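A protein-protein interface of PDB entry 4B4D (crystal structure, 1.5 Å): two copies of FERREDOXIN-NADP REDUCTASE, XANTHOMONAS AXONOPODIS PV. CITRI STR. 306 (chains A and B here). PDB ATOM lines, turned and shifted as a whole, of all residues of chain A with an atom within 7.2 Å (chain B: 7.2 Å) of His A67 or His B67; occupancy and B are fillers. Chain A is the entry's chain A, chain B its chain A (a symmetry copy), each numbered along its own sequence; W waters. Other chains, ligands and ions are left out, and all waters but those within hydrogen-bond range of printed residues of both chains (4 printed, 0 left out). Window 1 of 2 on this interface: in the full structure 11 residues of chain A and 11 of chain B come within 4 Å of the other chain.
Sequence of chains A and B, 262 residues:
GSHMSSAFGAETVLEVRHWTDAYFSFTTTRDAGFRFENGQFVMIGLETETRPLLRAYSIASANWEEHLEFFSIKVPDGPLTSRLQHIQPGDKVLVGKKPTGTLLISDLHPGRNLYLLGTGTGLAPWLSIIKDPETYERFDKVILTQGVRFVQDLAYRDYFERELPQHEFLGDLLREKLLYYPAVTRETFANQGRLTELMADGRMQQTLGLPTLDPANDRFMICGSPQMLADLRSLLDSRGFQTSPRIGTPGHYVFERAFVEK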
ATOM      1  N   LEU A  14     -18.746  -3.189  -0.515  1.00  0.00           N
ATOM      2  CA  LEU A  14     -17.800  -3.230   0.594  1.00  0.00           C
ATOM      3  C   LEU A  14     -17.703  -4.637   1.171  1.00  0.00           C
ATOM      4  O   LEU A  14     -16.672  -5.295   1.050  1.00  0.00           O
ATOM      5  CB  LEU A  14     -18.167  -2.184   1.657  1.00  0.00           C
ATOM      6  CG  LEU A  14     -18.140  -0.740   1.133  1.00  0.00           C
ATOM      7  CD1 LEU A  14     -18.560   0.263   2.189  1.00  0.00           C
ATOM      8  CD2 LEU A  14     -16.759  -0.400   0.572  1.00  0.00           C
ATOM      9  N   GLU A  15     -18.782  -5.103   1.781  1.00  0.00           N
ATOM     10  CA  GLU A  15     -18.818  -6.439   2.343  1.00  0.00           C
ATOM     11  C   GLU A  15     -19.983  -7.205   1.751  1.00  0.00           C
ATOM     12  O   GLU A  15     -20.977  -6.608   1.322  1.00  0.00           O
ATOM     13  CB  GLU A  15     -18.955  -6.382   3.859  1.00  0.00           C
ATOM     14  CG  GLU A  15     -17.673  -5.992   4.576  1.00  0.00           C
ATOM     15  CD  GLU A  15     -17.812  -6.041   6.081  1.00  0.00           C
ATOM     16  OE1 GLU A  15     -18.508  -5.176   6.651  1.00  0.00           O
ATOM     17  OE2 GLU A  15     -17.217  -6.943   6.702  1.00  0.00           O
ATOM     18  N   THR A  27     -23.050  -4.593   1.594  1.00  0.00           N
ATOM     19  CA  THR A  27     -23.010  -3.177   1.891  1.00  0.00           C
ATOM     20  C   THR A  27     -22.327  -2.423   0.763  1.00  0.00           C
ATOM     21  O   THR A  27     -21.510  -2.992   0.039  1.00  0.00           O
ATOM     22  CB  THR A  27     -22.268  -2.899   3.206  1.00  0.00           C
ATOM     23  OG1 THR A  27     -20.998  -3.563   3.178  1.00  0.00           O
ATOM     24  CG2 THR A  27     -23.071  -3.421   4.379  1.00  0.00           C
ATOM     25  N   THR A  28     -22.693  -1.161   0.605  1.00  0.00           N
ATOM     26  CA  THR A  28     -22.067  -0.298  -0.400  1.00  0.00           C
ATOM     27  C   THR A  28     -21.696   1.044   0.185  1.00  0.00           C
ATOM     28  O   THR A  28     -22.191   1.445   1.239  1.00  0.00           O
ATOM     29  CB  THR A  28     -22.982  -0.006  -1.613  1.00  0.00           C
ATOM     30  OG1 THR A  28     -24.009   0.914  -1.228  1.00  0.00           O
ATOM     31  CG2 THR A  28     -23.585  -1.287  -2.202  1.00  0.00           C
ATOM     32  N   THR A  29     -20.844   1.763  -0.539  1.00  0.00           N
ATOM     33  CA  THR A  29     -20.618   3.163  -0.236  1.00  0.00           C
ATOM     34  C   THR A  29     -21.906   3.967  -0.428  1.00  0.00           C
ATOM     35  O   THR A  29     -22.866   3.517  -1.062  1.00  0.00           O
ATOM     36  CB  THR A  29     -19.488   3.755  -1.094  1.00  0.00           C
ATOM     37  OG1 THR A  29     -19.743   3.466  -2.471  1.00  0.00           O
ATOM     38  CG2 THR A  29     -18.170   3.126  -0.712  1.00  0.00           C
ATOM     39  N   ARG A  30     -21.917   5.160   0.136  1.00  0.00           N
ATOM     40  CA  ARG A  30     -23.089   5.999   0.111  1.00  0.00           C
ATOM     41  C   ARG A  30     -22.659   7.367  -0.374  1.00  0.00           C
ATOM     42  O   ARG A  30     -21.646   7.886   0.096  1.00  0.00           O
ATOM     43  CB  ARG A  30     -23.680   6.073   1.519  1.00  0.00           C
ATOM     44  CG  ARG A  30     -24.904   6.950   1.640  1.00  0.00           C
ATOM     45  CD  ARG A  30     -25.424   6.930   3.064  1.00  0.00           C
ATOM     46  NE  ARG A  30     -26.476   7.916   3.243  1.00  0.00           N
ATOM     47  CZ  ARG A  30     -27.213   8.049   4.344  1.00  0.00           C
ATOM     48  NH1 ARG A  30     -27.029   7.243   5.382  1.00  0.00           N
ATOM     49  NH2 ARG A  30     -28.140   8.988   4.409  1.00  0.00           N
ATOM     50  N   PHE A  36     -32.337   9.609   3.017  1.00  0.00           N
ATOM     51  CA  PHE A  36     -33.556   8.794   2.979  1.00  0.00           C
ATOM     52  C   PHE A  36     -34.240   8.718   4.336  1.00  0.00           C
ATOM     53  O   PHE A  36     -33.632   9.012   5.367  1.00  0.00           O
ATOM     54  CB  PHE A  36     -33.274   7.391   2.416  1.00  0.00           C
ATOM     55  CG  PHE A  36     -32.406   6.519   3.290  1.00  0.00           C
ATOM     56  CD1 PHE A  36     -31.014   6.618   3.250  1.00  0.00           C
ATOM     57  CD2 PHE A  36     -32.978   5.552   4.118  1.00  0.00           C
ATOM     58  CE1 PHE A  36     -30.216   5.801   4.041  1.00  0.00           C
ATOM     59  CE2 PHE A  36     -32.184   4.733   4.905  1.00  0.00           C
ATOM     60  CZ  PHE A  36     -30.802   4.850   4.867  1.00  0.00           C
ATOM     61  N   ILE A  59     -33.791  -0.154   1.543  1.00  0.00           N
ATOM     62  CA  ILE A  59     -32.485   0.174   2.131  1.00  0.00           C
ATOM     63  C   ILE A  59     -32.425  -0.463   3.526  1.00  0.00           C
ATOM     64  O   ILE A  59     -33.155  -0.061   4.446  1.00  0.00           O
ATOM     65  CB  ILE A  59     -32.218   1.689   2.179  1.00  0.00           C
ATOM     66  CG1 ILE A  59     -32.356   2.305   0.780  1.00  0.00           C
ATOM     67  CG2 ILE A  59     -30.831   1.951   2.777  1.00  0.00           C
ATOM     68  CD1 ILE A  59     -32.681   3.789   0.769  1.00  0.00           C
ATOM     69  N   ALA A  60     -31.567  -1.470   3.679  1.00  0.00           N
ATOM     70  CA  ALA A  60     -31.532  -2.271   4.909  1.00  0.00           C
ATOM     71  C   ALA A  60     -30.551  -1.708   5.932  1.00  0.00           C
ATOM     72  O   ALA A  60     -29.820  -2.456   6.593  1.00  0.00           O
ATOM     73  CB  ALA A  60     -31.195  -3.720   4.598  1.00  0.00           C
ATOM     74  N   SER A  61     -30.558  -0.393   6.061  1.00  0.00           N
ATOM     75  CA  SER A  61     -29.681   0.313   6.991  1.00  0.00           C
ATOM     76  C   SER A  61     -30.355   1.607   7.401  1.00  0.00           C
ATOM     77  O   SER A  61     -31.302   2.045   6.756  1.00  0.00           O
ATOM     78  CB  SER A  61     -28.308   0.579   6.355  1.00  0.00           C
ATOM     79  OG  SER A  61     -28.415   1.257   5.106  1.00  0.00           O
ATOM     80  N   ALA A  62     -29.893   2.202   8.500  1.00  0.00           N
ATOM     81  CA  ALA A  62     -30.496   3.437   8.978  1.00  0.00           C
ATOM     82  C   ALA A  62     -29.821   4.647   8.341  1.00  0.00           C
ATOM     83  O   ALA A  62     -28.628   4.590   8.016  1.00  0.00           O
ATOM     84  CB  ALA A  62     -30.406   3.521  10.495  1.00  0.00           C
ATOM     85  N   ASN A  63     -30.573   5.731   8.207  1.00  0.00           N
ATOM     86  CA  ASN A  63     -30.102   6.935   7.510  1.00  0.00           C
ATOM     87  C   ASN A  63     -28.946   7.666   8.190  1.00  0.00           C
ATOM     88  O   ASN A  63     -28.292   8.496   7.558  1.00  0.00           O
ATOM     89  CB  ASN A  63     -31.248   7.892   7.137  1.00  0.00           C
ATOM     90  CG  ASN A  63     -32.046   8.372   8.331  1.00  0.00           C
ATOM     91  OD1 ASN A  63     -31.654   8.172   9.478  1.00  0.00           O
ATOM     92  ND2 ASN A  63     -33.179   9.016   8.065  1.00  0.00           N
ATOM     93  N   TRP A  64     -28.708   7.357   9.462  1.00  0.00           N
ATOM     94  CA  TRP A  64     -27.571   7.936  10.186  1.00  0.00           C
ATOM     95  C   TRP A  64     -26.287   7.193   9.916  1.00  0.00           C
ATOM     96  O   TRP A  64     -25.199   7.716  10.190  1.00  0.00           O
ATOM     97  CB  TRP A  64     -27.858   8.042  11.695  1.00  0.00           C
ATOM     98  CG  TRP A  64     -28.056   6.717  12.386  1.00  0.00           C
ATOM     99  CD1 TRP A  64     -29.264   6.119  12.735  1.00  0.00           C
ATOM    100  CD2 TRP A  64     -27.023   5.765  12.812  1.00  0.00           C
ATOM    101  NE1 TRP A  64     -29.050   4.907  13.340  1.00  0.00           N
ATOM    102  CE2 TRP A  64     -27.731   4.633  13.414  1.00  0.00           C
ATOM    103  CE3 TRP A  64     -25.629   5.741  12.759  1.00  0.00           C
ATOM    104  CZ2 TRP A  64     -27.058   3.534  13.931  1.00  0.00           C
ATOM    105  CZ3 TRP A  64     -24.960   4.632  13.283  1.00  0.00           C
ATOM    106  CH2 TRP A  64     -25.660   3.554  13.859  1.00  0.00           C
ATOM    107  N   GLU A  65     -26.379   5.981   9.366  1.00  0.00           N
ATOM    108  CA  GLU A  65     -25.194   5.144   9.111  1.00  0.00           C
ATOM    109  C   GLU A  65     -24.400   5.592   7.879  1.00  0.00           C
ATOM    110  O   GLU A  65     -24.965   6.160   6.943  1.00  0.00           O
ATOM    111  CB  GLU A  65     -25.566   3.660   9.002  1.00  0.00           C
ATOM    112  CG  GLU A  65     -26.314   3.131  10.208  1.00  0.00           C
ATOM    113  CD  GLU A  65     -26.495   1.631  10.166  1.00  0.00           C
ATOM    114  OE1 GLU A  65     -25.551   0.896  10.508  1.00  0.00           O
ATOM    115  OE2 GLU A  65     -27.589   1.182   9.779  1.00  0.00           O
ATOM    116  N   GLU A  66     -23.095   5.317   7.890  1.00  0.00           N
ATOM    117  CA  GLU A  66     -22.177   5.794   6.848  1.00  0.00           C
ATOM    118  C   GLU A  66     -22.186   4.978   5.547  1.00  0.00           C
ATOM    119  O   GLU A  66     -21.699   5.446   4.521  1.00  0.00           O
ATOM    120  CB  GLU A  66     -20.747   5.874   7.400  1.00  0.00           C
ATOM    121  CG  GLU A  66     -20.514   7.035   8.364  1.00  0.00           C
ATOM    122  CD  GLU A  66     -19.118   7.037   8.979  1.00  0.00           C
ATOM    123  OE1 GLU A  66     -18.315   6.117   8.689  1.00  0.00           O
ATOM    124  OE2 GLU A  66     -18.819   7.967   9.762  1.00  0.00           O
ATOM    125  N   HIS A  67     -22.718   3.761   5.597  1.00  0.00           N
ATOM    126  CA  HIS A  67     -22.791   2.893   4.419  1.00  0.00           C
ATOM    127  C   HIS A  67     -24.223   2.523   4.192  1.00  0.00           C
ATOM    128  O   HIS A  67     -25.046   2.695   5.079  1.00  0.00           O
ATOM    129  CB  HIS A  67     -21.982   1.618   4.626  1.00  0.00           C
ATOM    130  CG  HIS A  67     -20.546   1.858   5.039  1.00  0.00           C
ATOM    131  ND1 HIS A  67     -19.732   2.711   4.383  1.00  0.00           N
ATOM    132  CD2 HIS A  67     -19.785   1.303   6.078  1.00  0.00           C
ATOM    133  CE1 HIS A  67     -18.516   2.713   4.973  1.00  0.00           C
ATOM    134  NE2 HIS A  67     -18.549   1.849   6.008  1.00  0.00           N
ATOM    135  N   LEU A  68     -24.526   2.011   3.003  1.00  0.00           N
ATOM    136  CA  LEU A  68     -25.831   1.408   2.728  1.00  0.00           C
ATOM    137  C   LEU A  68     -25.709  -0.106   2.874  1.00  0.00           C
ATOM    138  O   LEU A  68     -24.635  -0.667   2.641  1.00  0.00           O
ATOM    139  CB  LEU A  68     -26.300   1.769   1.313  1.00  0.00           C
ATOM    140  CG  LEU A  68     -26.455   3.264   1.010  1.00  0.00           C
ATOM    141  CD1 LEU A  68     -26.803   3.462  -0.455  1.00  0.00           C
ATOM    142  CD2 LEU A  68     -27.481   3.961   1.899  1.00  0.00           C
ATOM    143  N   GLU A  69     -26.797  -0.767   3.278  1.00  0.00           N
ATOM    144  CA  GLU A  69     -26.848  -2.223   3.271  1.00  0.00           C
ATOM    145  C   GLU A  69     -28.088  -2.665   2.510  1.00  0.00           C
ATOM    146  O   GLU A  69     -29.113  -1.978   2.549  1.00  0.00           O
ATOM    147  CB  GLU A  69     -26.856  -2.796   4.693  1.00  0.00           C
ATOM    148  CG  GLU A  69     -26.719  -4.312   4.751  1.00  0.00           C
ATOM    149  CD  GLU A  69     -26.445  -4.851   6.145  1.00  0.00           C
ATOM    150  OE1 GLU A  69     -26.066  -4.068   7.045  1.00  0.00           O
ATOM    151  OE2 GLU A  69     -26.590  -6.078   6.324  1.00  0.00           O
ATOM    152  N   LEU B  14     -11.706  -1.856   2.417  1.00  0.00           N
ATOM    153  CA  LEU B  14     -13.082  -1.441   2.170  1.00  0.00           C
ATOM    154  C   LEU B  14     -13.122  -0.084   1.478  1.00  0.00           C
ATOM    155  O   LEU B  14     -13.514   0.018   0.318  1.00  0.00           O
ATOM    156  CB  LEU B  14     -13.895  -1.460   3.473  1.00  0.00           C
ATOM    157  CG  LEU B  14     -13.984  -2.849   4.122  1.00  0.00           C
ATOM    158  CD1 LEU B  14     -14.745  -2.824   5.433  1.00  0.00           C
ATOM    159  CD2 LEU B  14     -14.600  -3.855   3.149  1.00  0.00           C
ATOM    160  N   GLU B  15     -12.699   0.954   2.184  1.00  0.00           N
ATOM    161  CA  GLU B  15     -12.663   2.289   1.622  1.00  0.00           C
ATOM    162  C   GLU B  15     -11.260   2.848   1.735  1.00  0.00           C
ATOM    163  O   GLU B  15     -10.491   2.448   2.618  1.00  0.00           O
ATOM    164  CB  GLU B  15     -13.643   3.206   2.345  1.00  0.00           C
ATOM    165  CG  GLU B  15     -15.096   2.964   1.972  1.00  0.00           C
ATOM    166  CD  GLU B  15     -16.035   3.952   2.628  1.00  0.00           C
ATOM    167  OE1 GLU B  15     -16.236   3.868   3.857  1.00  0.00           O
ATOM    168  OE2 GLU B  15     -16.582   4.813   1.913  1.00  0.00           O
ATOM    169  N   THR B  27      -9.932   1.750   5.381  1.00  0.00           N
ATOM    170  CA  THR B  27     -10.591   0.874   6.325  1.00  0.00           C
ATOM    171  C   THR B  27     -10.482  -0.569   5.865  1.00  0.00           C
ATOM    172  O   THR B  27     -10.342  -0.834   4.670  1.00  0.00           O
ATOM    173  CB  THR B  27     -12.072   1.240   6.493  1.00  0.00           C
ATOM    174  OG1 THR B  27     -12.683   1.330   5.199  1.00  0.00           O
ATOM    175  CG2 THR B  27     -12.204   2.576   7.194  1.00  0.00           C
ATOM    176  N   THR B  28     -10.514  -1.486   6.820  1.00  0.00           N
ATOM    177  CA  THR B  28     -10.485  -2.918   6.513  1.00  0.00           C
ATOM    178  C   THR B  28     -11.538  -3.667   7.296  1.00  0.00           C
ATOM    179  O   THR B  28     -12.067  -3.176   8.294  1.00  0.00           O
ATOM    180  CB  THR B  28      -9.133  -3.592   6.850  1.00  0.00           C
ATOM    181  OG1 THR B  28      -9.006  -3.727   8.269  1.00  0.00           O
ATOM    182  CG2 THR B  28      -7.944  -2.820   6.263  1.00  0.00           C
ATOM    183  N   THR B  29     -11.810  -4.891   6.856  1.00  0.00           N
ATOM    184  CA  THR B  29     -12.590  -5.808   7.664  1.00  0.00           C
ATOM    185  C   THR B  29     -11.856  -6.129   8.968  1.00  0.00           C
ATOM    186  O   THR B  29     -10.653  -5.892   9.114  1.00  0.00           O
ATOM    187  CB  THR B  29     -12.912  -7.104   6.901  1.00  0.00           C
ATOM    188  OG1 THR B  29     -11.702  -7.646   6.364  1.00  0.00           O
ATOM    189  CG2 THR B  29     -13.849  -6.807   5.755  1.00  0.00           C
ATOM    190  N   ARG B  30     -12.600  -6.665   9.917  1.00  0.00           N
ATOM    191  CA  ARG B  30     -12.069  -6.946  11.228  1.00  0.00           C
ATOM    192  C   ARG B  30     -12.426  -8.378  11.566  1.00  0.00           C
ATOM    193  O   ARG B  30     -13.571  -8.781  11.361  1.00  0.00           O
ATOM    194  CB  ARG B  30     -12.681  -5.972  12.234  1.00  0.00           C
ATOM    195  CG  ARG B  30     -12.230  -6.176  13.661  1.00  0.00           C
ATOM    196  CD  ARG B  30     -12.872  -5.144  14.567  1.00  0.00           C
ATOM    197  NE  ARG B  30     -12.605  -5.447  15.963  1.00  0.00           N
ATOM    198  CZ  ARG B  30     -12.928  -4.657  16.986  1.00  0.00           C
ATOM    199  NH1 ARG B  30     -13.525  -3.491  16.777  1.00  0.00           N
ATOM    200  NH2 ARG B  30     -12.650  -5.031  18.222  1.00  0.00           N
ATOM    201  N   PHE B  36      -9.125  -5.066  20.964  1.00  0.00           N
ATOM    202  CA  PHE B  36      -8.056  -4.120  21.303  1.00  0.00           C
ATOM    203  C   PHE B  36      -8.528  -3.038  22.263  1.00  0.00           C
ATOM    204  O   PHE B  36      -9.730  -2.815  22.422  1.00  0.00           O
ATOM    205  CB  PHE B  36      -7.427  -3.510  20.039  1.00  0.00           C
ATOM    206  CG  PHE B  36      -8.339  -2.601  19.253  1.00  0.00           C
ATOM    207  CD1 PHE B  36      -9.251  -3.117  18.330  1.00  0.00           C
ATOM    208  CD2 PHE B  36      -8.248  -1.214  19.389  1.00  0.00           C
ATOM    209  CE1 PHE B  36     -10.076  -2.277  17.592  1.00  0.00           C
ATOM    210  CE2 PHE B  36      -9.066  -0.374  18.651  1.00  0.00           C
ATOM    211  CZ  PHE B  36      -9.979  -0.901  17.748  1.00  0.00           C
ATOM    212  N   ILE B  59      -4.210   1.683  15.496  1.00  0.00           N
ATOM    213  CA  ILE B  59      -5.570   1.402  15.019  1.00  0.00           C
ATOM    214  C   ILE B  59      -6.386   2.698  15.138  1.00  0.00           C
ATOM    215  O   ILE B  59      -6.668   3.177  16.248  1.00  0.00           O
ATOM    216  CB  ILE B  59      -6.235   0.233  15.768  1.00  0.00           C
ATOM    217  CG1 ILE B  59      -5.360  -1.025  15.687  1.00  0.00           C
ATOM    218  CG2 ILE B  59      -7.636  -0.016  15.198  1.00  0.00           C
ATOM    219  CD1 ILE B  59      -5.587  -2.027  16.806  1.00  0.00           C
ATOM    220  N   ALA B  60      -6.750   3.274  13.994  1.00  0.00           N
ATOM    221  CA  ALA B  60      -7.385   4.597  13.967  1.00  0.00           C
ATOM    222  C   ALA B  60      -8.906   4.505  14.027  1.00  0.00           C
ATOM    223  O   ALA B  60      -9.618   5.235  13.327  1.00  0.00           O
ATOM    224  CB  ALA B  60      -6.953   5.377  12.736  1.00  0.00           C
ATOM    225  N   SER B  61      -9.387   3.614  14.877  1.00  0.00           N
ATOM    226  CA  SER B  61     -10.819   3.392  15.060  1.00  0.00           C
ATOM    227  C   SER B  61     -11.053   2.889  16.470  1.00  0.00           C
ATOM    228  O   SER B  61     -10.118   2.461  17.140  1.00  0.00           O
ATOM    229  CB  SER B  61     -11.355   2.398  14.019  1.00  0.00           C
ATOM    230  OG  SER B  61     -10.623   1.175  14.014  1.00  0.00           O
ATOM    231  N   ALA B  62     -12.297   2.974  16.939  1.00  0.00           N
ATOM    232  CA  ALA B  62     -12.605   2.534  18.291  1.00  0.00           C
ATOM    233  C   ALA B  62     -12.970   1.053  18.304  1.00  0.00           C
ATOM    234  O   ALA B  62     -13.507   0.539  17.315  1.00  0.00           O
ATOM    235  CB  ALA B  62     -13.743   3.362  18.874  1.00  0.00           C
ATOM    236  N   ASN B  63     -12.712   0.399  19.429  1.00  0.00           N
ATOM    237  CA  ASN B  63     -12.900  -1.052  19.557  1.00  0.00           C
ATOM    238  C   ASN B  63     -14.347  -1.528  19.463  1.00  0.00           C
ATOM    239  O   ASN B  63     -14.586  -2.719  19.263  1.00  0.00           O
ATOM    240  CB  ASN B  63     -12.180  -1.637  20.784  1.00  0.00           C
ATOM    241  CG  ASN B  63     -12.630  -1.029  22.096  1.00  0.00           C
ATOM    242  OD1 ASN B  63     -13.622  -0.307  22.152  1.00  0.00           O
ATOM    243  ND2 ASN B  63     -11.899  -1.324  23.167  1.00  0.00           N
ATOM    244  N   TRP B  64     -15.292  -0.604  19.609  1.00  0.00           N
ATOM    245  CA  TRP B  64     -16.713  -0.935  19.453  1.00  0.00           C
ATOM    246  C   TRP B  64     -17.141  -0.938  18.007  1.00  0.00           C
ATOM    247  O   TRP B  64     -18.200  -1.485  17.676  1.00  0.00           O
ATOM    248  CB  TRP B  64     -17.604  -0.015  20.307  1.00  0.00           C
ATOM    249  CG  TRP B  64     -17.554   1.439  19.915  1.00  0.00           C
ATOM    250  CD1 TRP B  64     -16.827   2.455  20.528  1.00  0.00           C
ATOM    251  CD2 TRP B  64     -18.239   2.087  18.790  1.00  0.00           C
ATOM    252  NE1 TRP B  64     -17.022   3.650  19.884  1.00  0.00           N
ATOM    253  CE2 TRP B  64     -17.853   3.499  18.833  1.00  0.00           C
ATOM    254  CE3 TRP B  64     -19.107   1.653  17.787  1.00  0.00           C
ATOM    255  CZ2 TRP B  64     -18.320   4.420  17.904  1.00  0.00           C
ATOM    256  CZ3 TRP B  64     -19.573   2.586  16.857  1.00  0.00           C
ATOM    257  CH2 TRP B  64     -19.190   3.940  16.917  1.00  0.00           C
ATOM    258  N   GLU B  65     -16.334  -0.348  17.124  1.00  0.00           N
ATOM    259  CA  GLU B  65     -16.680  -0.242  15.695  1.00  0.00           C
ATOM    260  C   GLU B  65     -16.480  -1.556  14.934  1.00  0.00           C
ATOM    261  O   GLU B  65     -15.631  -2.371  15.302  1.00  0.00           O
ATOM    262  CB  GLU B  65     -15.914   0.899  15.014  1.00  0.00           C
ATOM    263  CG  GLU B  65     -16.102   2.243  15.686  1.00  0.00           C
ATOM    264  CD  GLU B  65     -15.503   3.378  14.888  1.00  0.00           C
ATOM    265  OE1 GLU B  65     -16.135   3.843  13.923  1.00  0.00           O
ATOM    266  OE2 GLU B  65     -14.383   3.805  15.225  1.00  0.00           O
ATOM    267  N   GLU B  66     -17.258  -1.740  13.865  1.00  0.00           N
ATOM    268  CA  GLU B  66     -17.279  -2.998  13.109  1.00  0.00           C
ATOM    269  C   GLU B  66     -16.124  -3.180  12.113  1.00  0.00           C
ATOM    270  O   GLU B  66     -15.871  -4.292  11.656  1.00  0.00           O
ATOM    271  CB  GLU B  66     -18.621  -3.155  12.381  1.00  0.00           C
ATOM    272  CG  GLU B  66     -19.792  -3.498  13.298  1.00  0.00           C
ATOM    273  CD  GLU B  66     -21.132  -3.550  12.572  1.00  0.00           C
ATOM    274  OE1 GLU B  66     -21.179  -3.288  11.345  1.00  0.00           O
ATOM    275  OE2 GLU B  66     -22.152  -3.852  13.233  1.00  0.00           O
ATOM    276  N   HIS B  67     -15.444  -2.092  11.766  1.00  0.00           N
ATOM    277  CA  HIS B  67     -14.317  -2.142  10.831  1.00  0.00           C
ATOM    278  C   HIS B  67     -13.112  -1.574  11.512  1.00  0.00           C
ATOM    279  O   HIS B  67     -13.241  -0.917  12.534  1.00  0.00           O
ATOM    280  CB  HIS B  67     -14.606  -1.320   9.580  1.00  0.00           C
ATOM    281  CG  HIS B  67     -15.904  -1.679   8.890  1.00  0.00           C
ATOM    282  ND1 HIS B  67     -16.238  -2.951   8.584  1.00  0.00           N
ATOM    283  CD2 HIS B  67     -16.956  -0.872   8.434  1.00  0.00           C
ATOM    284  CE1 HIS B  67     -17.443  -2.962   7.972  1.00  0.00           C
ATOM    285  NE2 HIS B  67     -17.880  -1.690   7.878  1.00  0.00           N
ATOM    286  N   LEU B  68     -11.934  -1.824  10.947  1.00  0.00           N
ATOM    287  CA  LEU B  68     -10.709  -1.152  11.381  1.00  0.00           C
ATOM    288  C   LEU B  68     -10.433   0.016  10.439  1.00  0.00           C
ATOM    289  O   LEU B  68     -10.805  -0.034   9.263  1.00  0.00           O
ATOM    290  CB  LEU B  68      -9.528  -2.132  11.370  1.00  0.00           C
ATOM    291  CG  LEU B  68      -9.668  -3.371  12.262  1.00  0.00           C
ATOM    292  CD1 LEU B  68      -8.483  -4.297  12.050  1.00  0.00           C
ATOM    293  CD2 LEU B  68      -9.824  -3.039  13.744  1.00  0.00           C
ATOM    294  N   GLU B  69      -9.803   1.076  10.952  1.00  0.00           N
ATOM    295  CA  GLU B  69      -9.326   2.161  10.105  1.00  0.00           C
ATOM    296  C   GLU B  69      -7.854   2.401  10.400  1.00  0.00           C
ATOM    297  O   GLU B  69      -7.417   2.226  11.542  1.00  0.00           O
ATOM    298  CB  GLU B  69     -10.135   3.445  10.321  1.00  0.00           C
ATOM    299  CG  GLU B  69      -9.807   4.557   9.332  1.00  0.00           C
ATOM    300  CD  GLU B  69     -10.792   5.715   9.362  1.00  0.00           C
ATOM    301  OE1 GLU B  69     -11.900   5.567   9.926  1.00  0.00           O
ATOM    302  OE2 GLU B  69     -10.452   6.771   8.792  1.00  0.00           O
HETATM  303  O   HOH W   1     -19.691  -2.896   5.436  1.00  0.00           O
HETATM  304  O   HOH W   2     -15.426  -6.329   9.428  1.00  0.00           O
HETATM  305  O   HOH W   3     -15.306   1.809   5.579  1.00  0.00           O
HETATM  306  O   HOH W   4     -19.831   5.468   2.108  1.00  0.00           O
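Water W3 lies within hydrogen-bond range of OG1 of Thr B27 (2.7 Å), OE1 of Glu B15 (2.8 Å) and NE2 of His A67 (3.3 Å). Water W4 lies within hydrogen-bond range of the backbone NH of Arg A30 (2.9 Å), the backbone carbonyl oxygen of Glu A66 (3.1 Å) and the side-chain carboxylate of Glu B15 (3.3 Å). Water W2 lies within hydrogen-bond range of the backbone NH (N) of Arg B30 (2.9 Å), the backbone carbonyl oxygen (O) of Glu B66 (3.1 Å) and the side-chain carboxylate (OE2) of Glu A15 (3.3 Å).
Of the 18 printed residues of chain B, 4 touch a printed residue of chain A. Hydrophobic or aromatic side chains of chain B that line the printed part of chain A: Leu B14 and His B67. Along chain B the printed residues that touch a printed residue of chain A span positions 14 to 67. Of the 18 printed residues of chain A, 4 touch a printed residue of chain B. Printed residues of chain A that touch a printed residue of chain B: Leu A14, Glu A15, Thr A29 and His A67. Hydrophobic or aromatic side chains of chain A that line the printed part of chain B: Leu A14 and His A67.
Printed residues of chain B within 4 Å of Thr A29: Glu B15. His A67 touches just these residues of chain B: Glu B15 (2.8 Å) and His B67 (3.98 Å). Of the printed residues of chain A, Leu B14 touches Leu A14 (3.3 Å). His B67 touches just these residues of chain A: Glu A15 and His A67. The nearest residue of chain B that does not touch His A67 is Thr B27 (5.9 Å). The nearest residue of chain A that does not touch His B67 is Thr A27 (5.9 Å). The nearest printed residue of chain A that does not touch Thr B29 is Leu A14 (5.7 Å).
The backbone NH (N) of Leu A14 is in hydrogen-bond range of the backbone carbonyl oxygen (O) of Thr A27 (2.8 Å). The backbone NH (N) of Thr A27 lies within hydrogen-bond range of the backbone carbonyl oxygen (O) of Glu A15, 2.9 Å away. The backbone carbonyl oxygen (O) of Thr B27 sits at hydrogen-bond distance from the backbone NH (N) of Leu B14 (2.8 Å). O of Glu B15 lies within hydrogen-bond range of N of Thr B27 (2.9 Å).
Among the printed residues, pairs that only touch across the chains: His A67 with Glu B15, Glu A15 with His B67, Leu A14 with Leu B14, Thr A29 with Glu B15, Glu A15 with Thr B29 and His A67 with His B67.
Leu B14 touches its own counterpart, Leu A14. Glu A15 touches Thr B29, and with the chains exchanged Thr A29 touches Glu B15. Glu A15 touches His B67, and with the chains exchanged His A67 touches Glu B15. His A67 touches its own counterpart, His B67. 18 positions are printed for both chains. Of the 6 pairs that touch across the chains among the printed residues, 6 have their exchanged pair printed and touching as well.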
